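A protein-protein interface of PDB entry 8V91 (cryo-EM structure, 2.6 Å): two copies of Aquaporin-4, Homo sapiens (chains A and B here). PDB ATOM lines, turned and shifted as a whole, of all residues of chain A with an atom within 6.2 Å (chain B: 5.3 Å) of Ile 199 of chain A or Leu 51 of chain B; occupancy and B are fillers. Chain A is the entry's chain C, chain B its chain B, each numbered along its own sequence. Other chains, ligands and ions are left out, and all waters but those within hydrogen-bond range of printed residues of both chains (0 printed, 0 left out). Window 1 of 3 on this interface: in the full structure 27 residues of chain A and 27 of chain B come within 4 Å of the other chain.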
ATOM      1  N   SER A  74      -0.690 -15.536 -19.236  1.00  0.00           N
ATOM      2  CA  SER A  74      -0.406 -14.232 -19.827  1.00  0.00           C
ATOM      3  C   SER A  74       0.755 -14.306 -20.812  1.00  0.00           C
ATOM      4  O   SER A  74       0.669 -13.782 -21.928  1.00  0.00           O
ATOM      5  CB  SER A  74      -0.113 -13.212 -18.727  1.00  0.00           C
ATOM      6  OG  SER A  74      -1.196 -13.117 -17.820  1.00  0.00           O
ATOM      7  N   ILE A 165     -11.885  -1.997 -23.548  1.00  0.00           N
ATOM      8  CA  ILE A 165     -10.695  -1.254 -23.146  1.00  0.00           C
ATOM      9  C   ILE A 165      -9.418  -2.051 -23.391  1.00  0.00           C
ATOM     10  O   ILE A 165      -8.428  -1.505 -23.881  1.00  0.00           O
ATOM     11  CB  ILE A 165     -10.827  -0.824 -21.672  1.00  0.00           C
ATOM     12  CG1 ILE A 165     -11.961   0.193 -21.526  1.00  0.00           C
ATOM     13  CG2 ILE A 165      -9.524  -0.238 -21.163  1.00  0.00           C
ATOM     14  CD1 ILE A 165     -12.258   0.586 -20.102  1.00  0.00           C
ATOM     15  N   ILE A 166      -9.408  -3.347 -23.063  1.00  0.00           N
ATOM     16  CA  ILE A 166      -8.192  -4.133 -23.257  1.00  0.00           C
ATOM     17  C   ILE A 166      -7.868  -4.274 -24.738  1.00  0.00           C
ATOM     18  O   ILE A 166      -6.696  -4.394 -25.114  1.00  0.00           O
ATOM     19  CB  ILE A 166      -8.307  -5.508 -22.572  1.00  0.00           C
ATOM     20  CG1 ILE A 166      -9.481  -6.306 -23.140  1.00  0.00           C
ATOM     21  CG2 ILE A 166      -8.445  -5.342 -21.068  1.00  0.00           C
ATOM     22  CD1 ILE A 166      -9.658  -7.657 -22.497  1.00  0.00           C
ATOM     23  N   GLN A 169      -6.268  -0.678 -25.951  1.00  0.00           N
ATOM     24  CA  GLN A 169      -4.831  -0.522 -25.758  1.00  0.00           C
ATOM     25  C   GLN A 169      -4.041  -1.409 -26.711  1.00  0.00           C
ATOM     26  O   GLN A 169      -2.910  -1.068 -27.076  1.00  0.00           O
ATOM     27  CB  GLN A 169      -4.461  -0.813 -24.302  1.00  0.00           C
ATOM     28  CG  GLN A 169      -4.814  -2.211 -23.809  1.00  0.00           C
ATOM     29  CD  GLN A 169      -3.700  -3.219 -24.010  1.00  0.00           C
ATOM     30  OE1 GLN A 169      -2.687  -2.929 -24.644  1.00  0.00           O
ATOM     31  NE2 GLN A 169      -3.885  -4.417 -23.470  1.00  0.00           N
ATOM     32  N   GLY A 194       3.337  -7.987 -28.431  1.00  0.00           N
ATOM     33  CA  GLY A 194       3.163  -9.143 -27.567  1.00  0.00           C
ATOM     34  C   GLY A 194       2.935  -8.766 -26.115  1.00  0.00           C
ATOM     35  O   GLY A 194       2.101  -9.368 -25.434  1.00  0.00           O
ATOM     36  N   PHE A 195       3.670  -7.768 -25.621  1.00  0.00           N
ATOM     37  CA  PHE A 195       3.503  -7.342 -24.238  1.00  0.00           C
ATOM     38  C   PHE A 195       2.204  -6.580 -24.021  1.00  0.00           C
ATOM     39  O   PHE A 195       1.707  -6.538 -22.892  1.00  0.00           O
ATOM     40  CB  PHE A 195       4.693  -6.488 -23.803  1.00  0.00           C
ATOM     41  CG  PHE A 195       5.957  -7.274 -23.602  1.00  0.00           C
ATOM     42  CD1 PHE A 195       5.908  -8.582 -23.155  1.00  0.00           C
ATOM     43  CD2 PHE A 195       7.191  -6.705 -23.858  1.00  0.00           C
ATOM     44  CE1 PHE A 195       7.066  -9.310 -22.970  1.00  0.00           C
ATOM     45  CE2 PHE A 195       8.353  -7.429 -23.672  1.00  0.00           C
ATOM     46  CZ  PHE A 195       8.290  -8.733 -23.228  1.00  0.00           C
ATOM     47  N   SER A 196       1.649  -5.970 -25.070  1.00  0.00           N
ATOM     48  CA  SER A 196       0.334  -5.351 -24.952  1.00  0.00           C
ATOM     49  C   SER A 196      -0.742  -6.397 -24.688  1.00  0.00           C
ATOM     50  O   SER A 196      -1.681  -6.151 -23.924  1.00  0.00           O
ATOM     51  CB  SER A 196       0.013  -4.554 -26.216  1.00  0.00           C
ATOM     52  OG  SER A 196      -1.219  -3.871 -26.089  1.00  0.00           O
ATOM     53  N   VAL A 197      -0.627  -7.565 -25.323  1.00  0.00           N
ATOM     54  CA  VAL A 197      -1.571  -8.649 -25.068  1.00  0.00           C
ATOM     55  C   VAL A 197      -1.385  -9.199 -23.659  1.00  0.00           C
ATOM     56  O   VAL A 197      -2.357  -9.538 -22.976  1.00  0.00           O
ATOM     57  CB  VAL A 197      -1.415  -9.752 -26.132  1.00  0.00           C
ATOM     58  CG1 VAL A 197      -2.209 -10.989 -25.746  1.00  0.00           C
ATOM     59  CG2 VAL A 197      -1.843  -9.243 -27.494  1.00  0.00           C
ATOM     60  N   ALA A 198      -0.132  -9.290 -23.202  1.00  0.00           N
ATOM     61  CA  ALA A 198       0.141  -9.879 -21.894  1.00  0.00           C
ATOM     62  C   ALA A 198      -0.499  -9.074 -20.771  1.00  0.00           C
ATOM     63  O   ALA A 198      -1.101  -9.647 -19.856  1.00  0.00           O
ATOM     64  CB  ALA A 198       1.649  -9.997 -21.677  1.00  0.00           C
ATOM     65  N   ILE A 199      -0.387  -7.745 -20.819  1.00  0.00           N
ATOM     66  CA  ILE A 199      -0.980  -6.927 -19.764  1.00  0.00           C
ATOM     67  C   ILE A 199      -2.500  -6.982 -19.827  1.00  0.00           C
ATOM     68  O   ILE A 199      -3.176  -6.800 -18.807  1.00  0.00           O
ATOM     69  CB  ILE A 199      -0.456  -5.480 -19.834  1.00  0.00           C
ATOM     70  CG1 ILE A 199      -0.938  -4.782 -21.103  1.00  0.00           C
ATOM     71  CG2 ILE A 199       1.053  -5.465 -19.767  1.00  0.00           C
ATOM     72  CD1 ILE A 199      -0.475  -3.352 -21.215  1.00  0.00           C
ATOM     73  N   GLY A 200      -3.067  -7.219 -21.011  1.00  0.00           N
ATOM     74  CA  GLY A 200      -4.498  -7.447 -21.095  1.00  0.00           C
ATOM     75  C   GLY A 200      -4.914  -8.720 -20.384  1.00  0.00           C
ATOM     76  O   GLY A 200      -5.976  -8.777 -19.761  1.00  0.00           O
ATOM     77  N   HIS A 201      -4.082  -9.760 -20.472  1.00  0.00           N
ATOM     78  CA  HIS A 201      -4.342 -10.993 -19.740  1.00  0.00           C
ATOM     79  C   HIS A 201      -3.993 -10.861 -18.264  1.00  0.00           C
ATOM     80  O   HIS A 201      -4.660 -11.464 -17.417  1.00  0.00           O
ATOM     81  CB  HIS A 201      -3.557 -12.147 -20.360  1.00  0.00           C
ATOM     82  CG  HIS A 201      -4.250 -12.788 -21.519  1.00  0.00           C
ATOM     83  ND1 HIS A 201      -4.230 -12.247 -22.785  1.00  0.00           N
ATOM     84  CD2 HIS A 201      -4.992 -13.917 -21.603  1.00  0.00           C
ATOM     85  CE1 HIS A 201      -4.923 -13.020 -23.603  1.00  0.00           C
ATOM     86  NE2 HIS A 201      -5.397 -14.039 -22.910  1.00  0.00           N
ATOM     87  N   LEU A 202      -2.965 -10.075 -17.937  1.00  0.00           N
ATOM     88  CA  LEU A 202      -2.595  -9.864 -16.543  1.00  0.00           C
ATOM     89  C   LEU A 202      -3.695  -9.155 -15.766  1.00  0.00           C
ATOM     90  O   LEU A 202      -3.666  -9.151 -14.532  1.00  0.00           O
ATOM     91  CB  LEU A 202      -1.298  -9.057 -16.463  1.00  0.00           C
ATOM     92  CG  LEU A 202       0.001  -9.771 -16.854  1.00  0.00           C
ATOM     93  CD1 LEU A 202       1.083  -8.762 -17.195  1.00  0.00           C
ATOM     94  CD2 LEU A 202       0.480 -10.709 -15.768  1.00  0.00           C
ATOM     95  N   PHE A 203      -4.659  -8.558 -16.463  1.00  0.00           N
ATOM     96  CA  PHE A 203      -5.764  -7.828 -15.858  1.00  0.00           C
ATOM     97  C   PHE A 203      -7.081  -8.589 -15.893  1.00  0.00           C
ATOM     98  O   PHE A 203      -7.714  -8.773 -14.850  1.00  0.00           O
ATOM     99  CB  PHE A 203      -5.931  -6.478 -16.572  1.00  0.00           C
ATOM    100  CG  PHE A 203      -7.193  -5.744 -16.211  1.00  0.00           C
ATOM    101  CD1 PHE A 203      -7.598  -5.620 -14.894  1.00  0.00           C
ATOM    102  CD2 PHE A 203      -7.981  -5.184 -17.201  1.00  0.00           C
ATOM    103  CE1 PHE A 203      -8.761  -4.948 -14.575  1.00  0.00           C
ATOM    104  CE2 PHE A 203      -9.142  -4.512 -16.887  1.00  0.00           C
ATOM    105  CZ  PHE A 203      -9.533  -4.394 -15.574  1.00  0.00           C
ATOM    106  N   ALA A 204      -7.512  -9.047 -17.069  1.00  0.00           N
ATOM    107  CA  ALA A 204      -8.903  -9.416 -17.297  1.00  0.00           C
ATOM    108  C   ALA A 204      -9.109 -10.909 -17.544  1.00  0.00           C
ATOM    109  O   ALA A 204      -9.993 -11.291 -18.311  1.00  0.00           O
ATOM    110  CB  ALA A 204      -9.468  -8.613 -18.467  1.00  0.00           C
ATOM    111  N   LEU B  46      -4.626   7.055 -17.498  1.00  0.00           N
ATOM    112  CA  LEU B  46      -5.860   6.360 -17.137  1.00  0.00           C
ATOM    113  C   LEU B  46      -5.760   4.865 -17.414  1.00  0.00           C
ATOM    114  O   LEU B  46      -6.181   4.045 -16.591  1.00  0.00           O
ATOM    115  CB  LEU B  46      -7.035   6.975 -17.899  1.00  0.00           C
ATOM    116  CG  LEU B  46      -8.485   6.561 -17.633  1.00  0.00           C
ATOM    117  CD1 LEU B  46      -9.408   7.676 -18.080  1.00  0.00           C
ATOM    118  CD2 LEU B  46      -8.859   5.275 -18.353  1.00  0.00           C
ATOM    119  N   ILE B  47      -5.221   4.492 -18.576  1.00  0.00           N
ATOM    120  CA  ILE B  47      -5.097   3.079 -18.914  1.00  0.00           C
ATOM    121  C   ILE B  47      -4.127   2.389 -17.964  1.00  0.00           C
ATOM    122  O   ILE B  47      -4.324   1.227 -17.587  1.00  0.00           O
ATOM    123  CB  ILE B  47      -4.669   2.921 -20.386  1.00  0.00           C
ATOM    124  CG1 ILE B  47      -5.864   3.135 -21.315  1.00  0.00           C
ATOM    125  CG2 ILE B  47      -4.059   1.552 -20.635  1.00  0.00           C
ATOM    126  CD1 ILE B  47      -5.557   4.010 -22.507  1.00  0.00           C
ATOM    127  N   PHE B  48      -3.075   3.099 -17.549  1.00  0.00           N
ATOM    128  CA  PHE B  48      -2.084   2.508 -16.657  1.00  0.00           C
ATOM    129  C   PHE B  48      -2.703   2.119 -15.319  1.00  0.00           C
ATOM    130  O   PHE B  48      -2.412   1.043 -14.786  1.00  0.00           O
ATOM    131  CB  PHE B  48      -0.923   3.483 -16.459  1.00  0.00           C
ATOM    132  CG  PHE B  48       0.008   3.108 -15.341  1.00  0.00           C
ATOM    133  CD1 PHE B  48       0.696   1.907 -15.366  1.00  0.00           C
ATOM    134  CD2 PHE B  48       0.202   3.962 -14.269  1.00  0.00           C
ATOM    135  CE1 PHE B  48       1.555   1.563 -14.340  1.00  0.00           C
ATOM    136  CE2 PHE B  48       1.058   3.623 -13.242  1.00  0.00           C
ATOM    137  CZ  PHE B  48       1.735   2.423 -13.278  1.00  0.00           C
ATOM    138  N   VAL B  49      -3.560   2.976 -14.762  1.00  0.00           N
ATOM    139  CA  VAL B  49      -4.198   2.663 -13.486  1.00  0.00           C
ATOM    140  C   VAL B  49      -5.136   1.471 -13.628  1.00  0.00           C
ATOM    141  O   VAL B  49      -5.078   0.520 -12.841  1.00  0.00           O
ATOM    142  CB  VAL B  49      -4.940   3.893 -12.935  1.00  0.00           C
ATOM    143  CG1 VAL B  49      -5.974   3.470 -11.918  1.00  0.00           C
ATOM    144  CG2 VAL B  49      -3.965   4.824 -12.274  1.00  0.00           C
ATOM    145  N   LEU B  50      -6.009   1.501 -14.637  1.00  0.00           N
ATOM    146  CA  LEU B  50      -7.050   0.484 -14.741  1.00  0.00           C
ATOM    147  C   LEU B  50      -6.459  -0.905 -14.938  1.00  0.00           C
ATOM    148  O   LEU B  50      -6.903  -1.873 -14.309  1.00  0.00           O
ATOM    149  CB  LEU B  50      -8.004   0.832 -15.882  1.00  0.00           C
ATOM    150  CG  LEU B  50      -9.053  -0.213 -16.251  1.00  0.00           C
ATOM    151  CD1 LEU B  50      -9.979  -0.477 -15.081  1.00  0.00           C
ATOM    152  CD2 LEU B  50      -9.841   0.251 -17.456  1.00  0.00           C
ATOM    153  N   LEU B  51      -5.448  -1.027 -15.800  1.00  0.00           N
ATOM    154  CA  LEU B  51      -4.855  -2.336 -16.048  1.00  0.00           C
ATOM    155  C   LEU B  51      -3.976  -2.782 -14.885  1.00  0.00           C
ATOM    156  O   LEU B  51      -4.026  -3.948 -14.478  1.00  0.00           O
ATOM    157  CB  LEU B  51      -4.054  -2.311 -17.351  1.00  0.00           C
ATOM    158  CG  LEU B  51      -4.756  -2.810 -18.618  1.00  0.00           C
ATOM    159  CD1 LEU B  51      -6.081  -2.101 -18.841  1.00  0.00           C
ATOM    160  CD2 LEU B  51      -3.853  -2.641 -19.826  1.00  0.00           C
ATOM    161  N   SER B  52      -3.166  -1.873 -14.337  1.00  0.00           N
ATOM    162  CA  SER B  52      -2.206  -2.265 -13.308  1.00  0.00           C
ATOM    163  C   SER B  52      -2.884  -2.511 -11.964  1.00  0.00           C
ATOM    164  O   SER B  52      -2.560  -3.484 -11.273  1.00  0.00           O
ATOM    165  CB  SER B  52      -1.122  -1.199 -13.171  1.00  0.00           C
ATOM    166  OG  SER B  52      -0.396  -1.054 -14.380  1.00  0.00           O
ATOM    167  N   LEU B  53      -3.816  -1.640 -11.569  1.00  0.00           N
ATOM    168  CA  LEU B  53      -4.491  -1.833 -10.288  1.00  0.00           C
ATOM    169  C   LEU B  53      -5.413  -3.044 -10.317  1.00  0.00           C
ATOM    170  O   LEU B  53      -5.621  -3.685  -9.282  1.00  0.00           O
ATOM    171  CB  LEU B  53      -5.279  -0.581  -9.900  1.00  0.00           C
ATOM    172  CG  LEU B  53      -4.470   0.658  -9.518  1.00  0.00           C
ATOM    173  CD1 LEU B  53      -5.366   1.695  -8.863  1.00  0.00           C
ATOM    174  CD2 LEU B  53      -3.316   0.289  -8.607  1.00  0.00           C
ATOM    175  N   GLY B  54      -5.976  -3.365 -11.483  1.00  0.00           N
ATOM    176  CA  GLY B  54      -6.814  -4.545 -11.590  1.00  0.00           C
ATOM    177  C   GLY B  54      -6.060  -5.831 -11.324  1.00  0.00           C
ATOM    178  O   GLY B  54      -6.626  -6.787 -10.789  1.00  0.00           O
ATOM    179  N   SER B  55      -4.778  -5.879 -11.693  1.00  0.00           N
ATOM    180  CA  SER B  55      -3.973  -7.067 -11.439  1.00  0.00           C
ATOM    181  C   SER B  55      -3.699  -7.276  -9.957  1.00  0.00           C
ATOM    182  O   SER B  55      -3.386  -8.400  -9.551  1.00  0.00           O
ATOM    183  CB  SER B  55      -2.652  -6.983 -12.200  1.00  0.00           C
ATOM    184  OG  SER B  55      -1.690  -6.250 -11.466  1.00  0.00           O
ATOM    185  N   LEU B  75       4.941  -7.449 -13.222  1.00  0.00           N
ATOM    186  CA  LEU B  75       4.949  -7.420 -14.681  1.00  0.00           C
ATOM    187  C   LEU B  75       3.822  -6.556 -15.230  1.00  0.00           C
ATOM    188  O   LEU B  75       4.013  -5.835 -16.215  1.00  0.00           O
ATOM    189  CB  LEU B  75       4.860  -8.837 -15.238  1.00  0.00           C
ATOM    190  CG  LEU B  75       6.142  -9.669 -15.169  1.00  0.00           C
ATOM    191  CD1 LEU B  75       6.157 -10.711 -16.274  1.00  0.00           C
ATOM    192  CD2 LEU B  75       7.379  -8.786 -15.245  1.00  0.00           C
ATOM    193  N   CYS B  76       2.638  -6.616 -14.616  1.00  0.00           N
ATOM    194  CA  CYS B  76       1.534  -5.787 -15.087  1.00  0.00           C
ATOM    195  C   CYS B  76       1.853  -4.307 -14.933  1.00  0.00           C
ATOM    196  O   CYS B  76       1.572  -3.509 -15.833  1.00  0.00           O
ATOM    197  CB  CYS B  76       0.249  -6.133 -14.339  1.00  0.00           C
ATOM    198  SG  CYS B  76      -1.204  -5.290 -14.989  1.00  0.00           S
ATOM    199  N   LEU B  79       5.174  -3.635 -17.412  1.00  0.00           N
ATOM    200  CA  LEU B  79       4.943  -3.665 -18.852  1.00  0.00           C
ATOM    201  C   LEU B  79       3.907  -2.639 -19.296  1.00  0.00           C
ATOM    202  O   LEU B  79       3.933  -2.210 -20.455  1.00  0.00           O
ATOM    203  CB  LEU B  79       4.517  -5.066 -19.291  1.00  0.00           C
ATOM    204  CG  LEU B  79       5.518  -6.199 -19.064  1.00  0.00           C
ATOM    205  CD1 LEU B  79       4.944  -7.519 -19.550  1.00  0.00           C
ATOM    206  CD2 LEU B  79       6.842  -5.898 -19.745  1.00  0.00           C
ATOM    207  N   SER B  80       2.987  -2.246 -18.412  1.00  0.00           N
ATOM    208  CA  SER B  80       2.007  -1.227 -18.779  1.00  0.00           C
ATOM    209  C   SER B  80       2.686   0.098 -19.092  1.00  0.00           C
ATOM    210  O   SER B  80       2.310   0.787 -20.047  1.00  0.00           O
ATOM    211  CB  SER B  80       0.981  -1.049 -17.662  1.00  0.00           C
ATOM    212  OG  SER B  80       0.151  -2.190 -17.549  1.00  0.00           O
ATOM    213  N   THR B  83       4.253  -0.246 -22.332  1.00  0.00           N
ATOM    214  CA  THR B  83       3.247  -0.153 -23.385  1.00  0.00           C
ATOM    215  C   THR B  83       2.796   1.288 -23.593  1.00  0.00           C
ATOM    216  O   THR B  83       2.609   1.726 -24.735  1.00  0.00           O
ATOM    217  CB  THR B  83       2.055  -1.049 -23.053  1.00  0.00           C
ATOM    218  OG1 THR B  83       2.503  -2.398 -22.877  1.00  0.00           O
ATOM    219  CG2 THR B  83       1.033  -1.012 -24.173  1.00  0.00           C
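The side-chain hydroxyl (OG) of Ser 55 of chain B lies close to the side-chain sulfur (SG) of Cys 76 of chain B, 3.7 Å away. OG of Ser 52 of chain B is in hydrogen-bond range of OG of Ser 80 of chain B, 3.4 Å away. O of Leu 79 of chain B sits at hydrogen-bond distance from OG1 of Thr 83 of chain B (2.8 Å). The backbone carbonyl oxygen (O) of Cys 76 of chain B is in hydrogen-bond range of the side-chain hydroxyl (OG) of Ser 52 of chain B, 3.5 Å away. The backbone carbonyl oxygen (O) of Cys 76 of chain B sits at hydrogen-bond distance from the side-chain hydroxyl (OG) of Ser 80 of chain B, 2.6 Å away. O of Ser 52 of chain B lies within hydrogen-bond range of OG of Ser 55 of chain B (2.9 Å).
Among the printed residues, pairs that only touch across the chains: Leu 202 of chain A with Ser 55 of chain B, Ile 199 of chain A with Leu 79 of chain B, Ile 199 of chain A with Thr 83 of chain B, Phe 203 of chain A with Gly 54 of chain B, Ile 165 of chain A with Leu 50 of chain B, Phe 203 of chain A with Leu 50 of chain B, Leu 202 of chain A with Cys 76 of chain B, Ile 199 of chain A with Leu 51 of chain B, Phe 203 of chain A with Leu 51 of chain B, Phe 195 of chain A with Leu 79 of chain B and Ile 199 of chain A with Ser 80 of chain B.
Ile 199 of chain A touches four residues of chain B. Printed residues of chain A within 4 Å of Leu 51 of chain B: Ile 199 and Phe 203. Printed residues of chain A within 4 Å of Ser 80 of chain B: Ile 199. Of the printed residues of chain B, Phe 195 of chain A touches Leu 79. The nearest residue of chain A that does not touch Leu 51 of chain B is Gln 169 of chain A (4.1 Å).
Of the 15 printed residues of chain B, 8 touch a printed residue of chain A. Hydrophobic or aromatic side chains of chain B within 4 Å of the printed part of chain A: Leu 50, Leu 51 and Leu 79. Hydrophobic or aromatic side chains of chain A within 4 Å of the printed part of chain B: Ile 165, Phe 195, Ile 199, Leu 202 and Phe 203. Among the printed residues, 11 pairs touch across the chains. Among the printed residues, no Asp or Glu carboxylate lies within 4 Å of a Lys or Arg side-chain nitrogen of the other chain.
No position is printed for both chains.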
